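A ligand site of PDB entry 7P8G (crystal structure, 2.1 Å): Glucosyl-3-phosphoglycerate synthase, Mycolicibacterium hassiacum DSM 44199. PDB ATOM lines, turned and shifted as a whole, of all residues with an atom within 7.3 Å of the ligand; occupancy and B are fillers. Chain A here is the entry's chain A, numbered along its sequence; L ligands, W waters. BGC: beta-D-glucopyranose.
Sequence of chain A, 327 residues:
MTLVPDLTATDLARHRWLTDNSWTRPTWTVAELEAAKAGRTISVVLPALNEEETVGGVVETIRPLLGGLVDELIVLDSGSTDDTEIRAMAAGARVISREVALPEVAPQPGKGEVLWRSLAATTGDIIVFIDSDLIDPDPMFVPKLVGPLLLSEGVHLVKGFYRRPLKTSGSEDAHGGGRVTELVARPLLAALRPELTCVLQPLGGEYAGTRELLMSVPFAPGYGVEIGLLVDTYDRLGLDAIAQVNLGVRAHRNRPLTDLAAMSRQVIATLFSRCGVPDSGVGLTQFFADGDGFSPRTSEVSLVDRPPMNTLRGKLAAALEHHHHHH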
ATOM      1  N   LYS A 111      31.933 -17.670  -2.134  1.00  0.00           N
ATOM      2  CA  LYS A 111      32.248 -18.432  -3.344  1.00  0.00           C
ATOM      3  C   LYS A 111      31.860 -17.673  -4.607  1.00  0.00           C
ATOM      4  O   LYS A 111      32.640 -17.615  -5.568  1.00  0.00           O
ATOM      5  CB  LYS A 111      31.529 -19.779  -3.274  1.00  0.00           C
ATOM      6  CG  LYS A 111      32.102 -20.879  -4.138  1.00  0.00           C
ATOM      7  CD  LYS A 111      31.145 -22.066  -4.014  1.00  0.00           C
ATOM      8  CE  LYS A 111      31.721 -23.356  -4.502  1.00  0.00           C
ATOM      9  NZ  LYS A 111      31.789 -24.335  -3.367  1.00  0.00           N
ATOM     10  N   GLY A 112      30.650 -17.091  -4.638  1.00  0.00           N
ATOM     11  CA  GLY A 112      30.207 -16.355  -5.814  1.00  0.00           C
ATOM     12  C   GLY A 112      31.204 -15.305  -6.251  1.00  0.00           C
ATOM     13  O   GLY A 112      31.503 -15.180  -7.441  1.00  0.00           O
ATOM     14  N   ASP A 131      34.479 -27.972  -7.536  1.00  0.00           N
ATOM     15  CA  ASP A 131      34.793 -27.746  -6.128  1.00  0.00           C
ATOM     16  C   ASP A 131      36.144 -28.372  -5.792  1.00  0.00           C
ATOM     17  O   ASP A 131      36.514 -29.427  -6.310  1.00  0.00           O
ATOM     18  CB  ASP A 131      33.692 -28.310  -5.232  1.00  0.00           C
ATOM     19  CG  ASP A 131      32.484 -27.366  -5.142  1.00  0.00           C
ATOM     20  OD1 ASP A 131      32.680 -26.162  -5.379  1.00  0.00           O
ATOM     21  OD2 ASP A 131      31.353 -27.811  -4.839  1.00  0.00           O
ATOM     22  N   ASP A 133      37.039 -29.171  -2.668  1.00  0.00           N
ATOM     23  CA  ASP A 133      36.930 -29.970  -1.460  1.00  0.00           C
ATOM     24  C   ASP A 133      36.524 -31.411  -1.734  1.00  0.00           C
ATOM     25  O   ASP A 133      36.299 -32.163  -0.784  1.00  0.00           O
ATOM     26  CB  ASP A 133      35.921 -29.341  -0.499  1.00  0.00           C
ATOM     27  CG  ASP A 133      34.519 -29.233  -1.094  1.00  0.00           C
ATOM     28  OD1 ASP A 133      34.353 -29.496  -2.306  1.00  0.00           O
ATOM     29  OD2 ASP A 133      33.589 -28.883  -0.351  1.00  0.00           O
ATOM     30  N   LEU A 134      36.436 -31.812  -2.999  1.00  0.00           N
ATOM     31  CA  LEU A 134      35.977 -33.152  -3.337  1.00  0.00           C
ATOM     32  C   LEU A 134      36.973 -34.196  -2.845  1.00  0.00           C
ATOM     33  O   LEU A 134      38.171 -34.102  -3.114  1.00  0.00           O
ATOM     34  CB  LEU A 134      35.783 -33.257  -4.840  1.00  0.00           C
ATOM     35  CG  LEU A 134      34.796 -32.270  -5.445  1.00  0.00           C
ATOM     36  CD1 LEU A 134      34.483 -32.668  -6.862  1.00  0.00           C
ATOM     37  CD2 LEU A 134      33.554 -32.208  -4.589  1.00  0.00           C
ATOM     38  N   ARG A 164      23.258 -41.368  -5.987  1.00  0.00           N
ATOM     39  CA  ARG A 164      23.556 -41.767  -4.625  1.00  0.00           C
ATOM     40  C   ARG A 164      23.740 -43.283  -4.546  1.00  0.00           C
ATOM     41  O   ARG A 164      23.107 -44.032  -5.302  1.00  0.00           O
ATOM     42  CB  ARG A 164      22.437 -41.316  -3.683  1.00  0.00           C
ATOM     43  CG  ARG A 164      22.290 -39.792  -3.580  1.00  0.00           C
ATOM     44  CD  ARG A 164      23.672 -39.127  -3.542  1.00  0.00           C
ATOM     45  NE  ARG A 164      23.628 -37.666  -3.545  1.00  0.00           N
ATOM     46  CZ  ARG A 164      24.689 -36.892  -3.690  1.00  0.00           C
ATOM     47  NH1 ARG A 164      25.895 -37.407  -3.860  1.00  0.00           N
ATOM     48  NH2 ARG A 164      24.543 -35.568  -3.646  1.00  0.00           N
ATOM     49  N   GLY A 178      21.670 -34.593  -0.228  1.00  0.00           N
ATOM     50  CA  GLY A 178      21.900 -33.239   0.286  1.00  0.00           C
ATOM     51  C   GLY A 178      20.607 -32.639   0.798  1.00  0.00           C
ATOM     52  O   GLY A 178      19.630 -32.514   0.037  1.00  0.00           O
ATOM     53  N   VAL A 180      19.758 -29.566   2.042  1.00  0.00           N
ATOM     54  CA  VAL A 180      19.358 -28.259   1.534  1.00  0.00           C
ATOM     55  C   VAL A 180      18.803 -28.410   0.123  1.00  0.00           C
ATOM     56  O   VAL A 180      17.775 -27.806  -0.225  1.00  0.00           O
ATOM     57  CB  VAL A 180      20.532 -27.259   1.584  1.00  0.00           C
ATOM     58  CG1 VAL A 180      20.057 -25.863   1.060  1.00  0.00           C
ATOM     59  CG2 VAL A 180      21.068 -27.126   2.981  1.00  0.00           C
ATOM     60  N   THR A 181      19.461 -29.215  -0.714  1.00  0.00           N
ATOM     61  CA  THR A 181      18.948 -29.502  -2.042  1.00  0.00           C
ATOM     62  C   THR A 181      17.549 -30.087  -1.987  1.00  0.00           C
ATOM     63  O   THR A 181      16.628 -29.607  -2.674  1.00  0.00           O
ATOM     64  CB  THR A 181      19.908 -30.455  -2.770  1.00  0.00           C
ATOM     65  OG1 THR A 181      21.129 -29.764  -3.076  1.00  0.00           O
ATOM     66  CG2 THR A 181      19.270 -31.004  -4.045  1.00  0.00           C
ATOM     67  N   GLN A 201      20.351 -31.884  -9.136  1.00  0.00           N
ATOM     68  CA  GLN A 201      21.137 -31.303  -8.054  1.00  0.00           C
ATOM     69  C   GLN A 201      21.420 -29.838  -8.400  1.00  0.00           C
ATOM     70  O   GLN A 201      22.521 -29.493  -8.856  1.00  0.00           O
ATOM     71  CB  GLN A 201      22.421 -32.125  -7.817  1.00  0.00           C
ATOM     72  CG  GLN A 201      22.124 -33.394  -7.029  1.00  0.00           C
ATOM     73  CD  GLN A 201      23.108 -34.542  -7.251  1.00  0.00           C
ATOM     74  OE1 GLN A 201      24.288 -34.338  -7.556  1.00  0.00           O
ATOM     75  NE2 GLN A 201      22.610 -35.762  -7.095  1.00  0.00           N
ATOM     76  N   PRO A 202      20.432 -28.953  -8.209  1.00  0.00           N
ATOM     77  CA  PRO A 202      20.598 -27.564  -8.639  1.00  0.00           C
ATOM     78  C   PRO A 202      21.735 -26.825  -7.946  1.00  0.00           C
ATOM     79  O   PRO A 202      22.297 -25.894  -8.534  1.00  0.00           O
ATOM     80  CB  PRO A 202      19.244 -26.925  -8.317  1.00  0.00           C
ATOM     81  CG  PRO A 202      18.664 -27.803  -7.240  1.00  0.00           C
ATOM     82  CD  PRO A 202      19.110 -29.184  -7.592  1.00  0.00           C
ATOM     83  N   LEU A 203      22.093 -27.215  -6.728  1.00  0.00           N
ATOM     84  CA  LEU A 203      23.153 -26.545  -5.987  1.00  0.00           C
ATOM     85  C   LEU A 203      24.554 -27.091  -6.282  1.00  0.00           C
ATOM     86  O   LEU A 203      25.505 -26.698  -5.601  1.00  0.00           O
ATOM     87  CB  LEU A 203      22.901 -26.637  -4.484  1.00  0.00           C
ATOM     88  CG  LEU A 203      21.543 -26.170  -3.959  1.00  0.00           C
ATOM     89  CD1 LEU A 203      21.584 -26.159  -2.440  1.00  0.00           C
ATOM     90  CD2 LEU A 203      21.185 -24.818  -4.502  1.00  0.00           C
ATOM     91  N   GLY A 204      24.700 -27.954  -7.284  1.00  0.00           N
ATOM     92  CA  GLY A 204      25.946 -28.688  -7.453  1.00  0.00           C
ATOM     93  C   GLY A 204      27.111 -27.790  -7.833  1.00  0.00           C
ATOM     94  O   GLY A 204      26.973 -26.849  -8.612  1.00  0.00           O
ATOM     95  N   GLY A 205      28.283 -28.109  -7.284  1.00  0.00           N
ATOM     96  CA  GLY A 205      29.480 -27.330  -7.566  1.00  0.00           C
ATOM     97  C   GLY A 205      30.194 -27.673  -8.859  1.00  0.00           C
ATOM     98  O   GLY A 205      31.100 -26.932  -9.250  1.00  0.00           O
ATOM     99  N   GLU A 206      29.804 -28.761  -9.535  1.00  0.00           N
ATOM    100  CA  GLU A 206      30.444 -29.166 -10.792  1.00  0.00           C
ATOM    101  C   GLU A 206      29.522 -28.780 -11.954  1.00  0.00           C
ATOM    102  O   GLU A 206      28.477 -29.395 -12.166  1.00  0.00           O
ATOM    103  CB  GLU A 206      30.721 -30.672 -10.794  1.00  0.00           C
ATOM    104  CG  GLU A 206      31.845 -31.104  -9.839  1.00  0.00           C
ATOM    105  CD  GLU A 206      31.513 -30.807  -8.383  1.00  0.00           C
ATOM    106  OE1 GLU A 206      30.579 -31.439  -7.833  1.00  0.00           O
ATOM    107  OE2 GLU A 206      32.152 -29.907  -7.801  1.00  0.00           O
ATOM    108  N   TYR A 207      29.923 -27.768 -12.712  1.00  0.00           N
ATOM    109  CA  TYR A 207      29.125 -27.363 -13.855  1.00  0.00           C
ATOM    110  C   TYR A 207      29.985 -26.581 -14.820  1.00  0.00           C
ATOM    111  O   TYR A 207      31.026 -26.024 -14.453  1.00  0.00           O
ATOM    112  CB  TYR A 207      27.889 -26.548 -13.432  1.00  0.00           C
ATOM    113  CG  TYR A 207      28.172 -25.384 -12.504  1.00  0.00           C
ATOM    114  CD1 TYR A 207      28.235 -25.566 -11.128  1.00  0.00           C
ATOM    115  CD2 TYR A 207      28.346 -24.095 -13.007  1.00  0.00           C
ATOM    116  CE1 TYR A 207      28.479 -24.503 -10.272  1.00  0.00           C
ATOM    117  CE2 TYR A 207      28.591 -23.025 -12.163  1.00  0.00           C
ATOM    118  CZ  TYR A 207      28.652 -23.228 -10.800  1.00  0.00           C
ATOM    119  OH  TYR A 207      28.904 -22.159  -9.963  1.00  0.00           O
ATOM    120  N   GLY A 222      28.258 -15.640  -2.313  1.00  0.00           N
ATOM    121  CA  GLY A 222      28.223 -16.696  -1.303  1.00  0.00           C
ATOM    122  C   GLY A 222      27.637 -17.981  -1.847  1.00  0.00           C
ATOM    123  O   GLY A 222      27.855 -18.360  -3.003  1.00  0.00           O
ATOM    124  N   TYR A 223      26.852 -18.643  -1.000  1.00  0.00           N
ATOM    125  CA  TYR A 223      26.199 -19.901  -1.330  1.00  0.00           C
ATOM    126  C   TYR A 223      25.047 -19.736  -2.321  1.00  0.00           C
ATOM    127  O   TYR A 223      24.491 -20.755  -2.764  1.00  0.00           O
ATOM    128  CB  TYR A 223      25.704 -20.543  -0.031  1.00  0.00           C
ATOM    129  CG  TYR A 223      26.891 -21.032   0.801  1.00  0.00           C
ATOM    130  CD1 TYR A 223      27.996 -21.599   0.176  1.00  0.00           C
ATOM    131  CD2 TYR A 223      26.916 -20.881   2.193  1.00  0.00           C
ATOM    132  CE1 TYR A 223      29.106 -22.048   0.905  1.00  0.00           C
ATOM    133  CE2 TYR A 223      28.016 -21.314   2.938  1.00  0.00           C
ATOM    134  CZ  TYR A 223      29.103 -21.893   2.288  1.00  0.00           C
ATOM    135  OH  TYR A 223      30.210 -22.327   3.001  1.00  0.00           O
ATOM    136  N   GLY A 224      24.687 -18.514  -2.701  1.00  0.00           N
ATOM    137  CA  GLY A 224      23.660 -18.379  -3.718  1.00  0.00           C
ATOM    138  C   GLY A 224      24.111 -18.650  -5.135  1.00  0.00           C
ATOM    139  O   GLY A 224      23.264 -18.819  -6.010  1.00  0.00           O
ATOM    140  N   VAL A 225      25.426 -18.728  -5.399  1.00  0.00           N
ATOM    141  CA  VAL A 225      25.920 -18.556  -6.758  1.00  0.00           C
ATOM    142  C   VAL A 225      25.370 -19.628  -7.700  1.00  0.00           C
ATOM    143  O   VAL A 225      24.955 -19.323  -8.827  1.00  0.00           O
ATOM    144  CB  VAL A 225      27.461 -18.511  -6.781  1.00  0.00           C
ATOM    145  CG1 VAL A 225      28.068 -19.812  -6.176  1.00  0.00           C
ATOM    146  CG2 VAL A 225      27.961 -18.282  -8.205  1.00  0.00           C
ATOM    147  N   GLU A 226      25.352 -20.914  -7.266  1.00  0.00           N
ATOM    148  CA  GLU A 226      24.958 -21.985  -8.187  1.00  0.00           C
ATOM    149  C   GLU A 226      23.487 -21.878  -8.569  1.00  0.00           C
ATOM    150  O   GLU A 226      23.139 -22.010  -9.745  1.00  0.00           O
ATOM    151  CB  GLU A 226      25.219 -23.376  -7.564  1.00  0.00           C
ATOM    152  CG  GLU A 226      26.670 -23.713  -7.393  1.00  0.00           C
ATOM    153  CD  GLU A 226      27.163 -23.375  -5.996  1.00  0.00           C
ATOM    154  OE1 GLU A 226      26.376 -22.809  -5.200  1.00  0.00           O
ATOM    155  OE2 GLU A 226      28.336 -23.698  -5.713  1.00  0.00           O
ATOM    156  N   ILE A 227      22.610 -21.702  -7.592  1.00  0.00           N
ATOM    157  CA  ILE A 227      21.193 -21.653  -7.926  1.00  0.00           C
ATOM    158  C   ILE A 227      20.878 -20.360  -8.672  1.00  0.00           C
ATOM    159  O   ILE A 227      20.033 -20.351  -9.574  1.00  0.00           O
ATOM    160  CB  ILE A 227      20.323 -21.838  -6.680  1.00  0.00           C
ATOM    161  CG1 ILE A 227      18.908 -22.244  -7.099  1.00  0.00           C
ATOM    162  CG2 ILE A 227      20.300 -20.554  -5.837  1.00  0.00           C
ATOM    163  CD1 ILE A 227      18.206 -23.091  -6.069  1.00  0.00           C
ATOM    164  N   HIS A 252      27.233 -38.576  -0.343  1.00  0.00           N
ATOM    165  CA  HIS A 252      27.156 -37.210   0.172  1.00  0.00           C
ATOM    166  C   HIS A 252      28.025 -37.041   1.419  1.00  0.00           C
ATOM    167  O   HIS A 252      28.012 -37.885   2.326  1.00  0.00           O
ATOM    168  CB  HIS A 252      25.706 -36.821   0.467  1.00  0.00           C
ATOM    169  CG  HIS A 252      25.486 -35.343   0.402  1.00  0.00           C
ATOM    170  ND1 HIS A 252      25.612 -34.632  -0.773  1.00  0.00           N
ATOM    171  CD2 HIS A 252      25.191 -34.438   1.361  1.00  0.00           C
ATOM    172  CE1 HIS A 252      25.375 -33.348  -0.541  1.00  0.00           C
ATOM    173  NE2 HIS A 252      25.123 -33.209   0.750  1.00  0.00           N
ATOM    174  N   ARG A 255      27.966 -32.253   6.646  1.00  0.00           N
ATOM    175  CA  ARG A 255      28.055 -30.879   7.112  1.00  0.00           C
ATOM    176  C   ARG A 255      27.160 -30.697   8.330  1.00  0.00           C
ATOM    177  O   ARG A 255      26.185 -31.433   8.500  1.00  0.00           O
ATOM    178  CB  ARG A 255      27.626 -29.882   6.024  1.00  0.00           C
ATOM    179  CG  ARG A 255      28.731 -29.432   5.078  1.00  0.00           C
ATOM    180  CD  ARG A 255      28.782 -30.279   3.808  1.00  0.00           C
ATOM    181  NE  ARG A 255      27.534 -30.261   3.049  1.00  0.00           N
ATOM    182  CZ  ARG A 255      27.169 -29.297   2.206  1.00  0.00           C
ATOM    183  NH1 ARG A 255      27.911 -28.216   2.025  1.00  0.00           N
ATOM    184  NH2 ARG A 255      26.027 -29.415   1.529  1.00  0.00           N
ATOM    185  N   MET A 263      23.309 -21.500   5.081  1.00  0.00           N
ATOM    186  CA  MET A 263      23.386 -21.700   3.633  1.00  0.00           C
ATOM    187  C   MET A 263      21.993 -21.664   3.013  1.00  0.00           C
ATOM    188  O   MET A 263      21.781 -21.031   1.963  1.00  0.00           O
ATOM    189  CB  MET A 263      24.082 -23.022   3.331  1.00  0.00           C
ATOM    190  CG  MET A 263      23.982 -23.448   1.892  1.00  0.00           C
ATOM    191  SD  MET A 263      24.490 -25.162   1.734  1.00  0.00           S
ATOM    192  CE  MET A 263      23.952 -25.505   0.073  1.00  0.00           C
ATOM    193  N   VAL A 267      20.420 -19.307  -0.007  1.00  0.00           N
ATOM    194  CA  VAL A 267      19.753 -19.896  -1.160  1.00  0.00           C
ATOM    195  C   VAL A 267      18.378 -19.262  -1.363  1.00  0.00           C
ATOM    196  O   VAL A 267      17.969 -18.951  -2.486  1.00  0.00           O
ATOM    197  CB  VAL A 267      19.640 -21.424  -0.994  1.00  0.00           C
ATOM    198  CG1 VAL A 267      18.633 -21.999  -1.969  1.00  0.00           C
ATOM    199  CG2 VAL A 267      21.007 -22.088  -1.189  1.00  0.00           C
HETATM  200  C2  BGC L   1      27.955 -27.959  -2.505  1.00  0.00           C
HETATM  201  C3  BGC L   1      28.728 -26.667  -2.847  1.00  0.00           C
HETATM  202  C4  BGC L   1      28.316 -25.453  -1.995  1.00  0.00           C
HETATM  203  C5  BGC L   1      26.802 -25.332  -1.839  1.00  0.00           C
HETATM  204  C6  BGC L   1      26.231 -24.051  -2.401  1.00  0.00           C
HETATM  205  C1  BGC L   1      26.552 -27.658  -1.999  1.00  0.00           C
HETATM  206  O1  BGC L   1      25.664 -28.655  -2.398  1.00  0.00           O
HETATM  207  O2  BGC L   1      28.674 -28.709  -1.532  1.00  0.00           O
HETATM  208  O3  BGC L   1      28.641 -26.403  -4.235  1.00  0.00           O
HETATM  209  O4  BGC L   1      28.905 -25.525  -0.702  1.00  0.00           O
HETATM  210  O5  BGC L   1      26.138 -26.406  -2.501  1.00  0.00           O
HETATM  211  O6  BGC L   1      27.199 -23.016  -2.440  1.00  0.00           O
HETATM  212  O   HOH W   1      31.648 -29.653  -2.736  1.00  0.00           O
HETATM  213  O   HOH W   2      24.600 -30.903  -4.816  1.00  0.00           O
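OD1 of Asp 131 is in salt-bridge range of NZ of Lys 111 (2.9 Å). The backbone NH of Asp 131 sits at hydrogen-bond distance from the side-chain carboxylate of Glu 206, 3.0 Å away.
Merely in contact with the ligand: Tyr 223, Met 263, Gly 205, Arg 255 and Lys 111. Hydrophobic or aromatic side chains that line the ligand: Leu 203, Tyr 223 and Met 263. Eight residues have an atom within 4 Å of the ligand: Lys 111, Asp 131, Leu 203, Gly 205, Tyr 223, Glu 226, Arg 255 and Met 263. The nearest printed residue that does not touch the ligand is Gly 204 (4.1 Å).
OD2 of Asp 131 lies within hydrogen-bond range of O3 of the ligand (3.1 Å). The backbone carbonyl oxygen (O) of Leu 203 sits at hydrogen-bond distance from an oxygen (O3) of the ligand, at 3.4 Å. OE1 of Glu 226 sits at hydrogen-bond distance from O6 of the ligand (2.9 Å).
Water W1 lies within hydrogen-bond range of OD1 of Asp 133 (2.7 Å), OD2 of Asp 131 (2.8 Å) and O2 of the ligand (3.3 Å).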
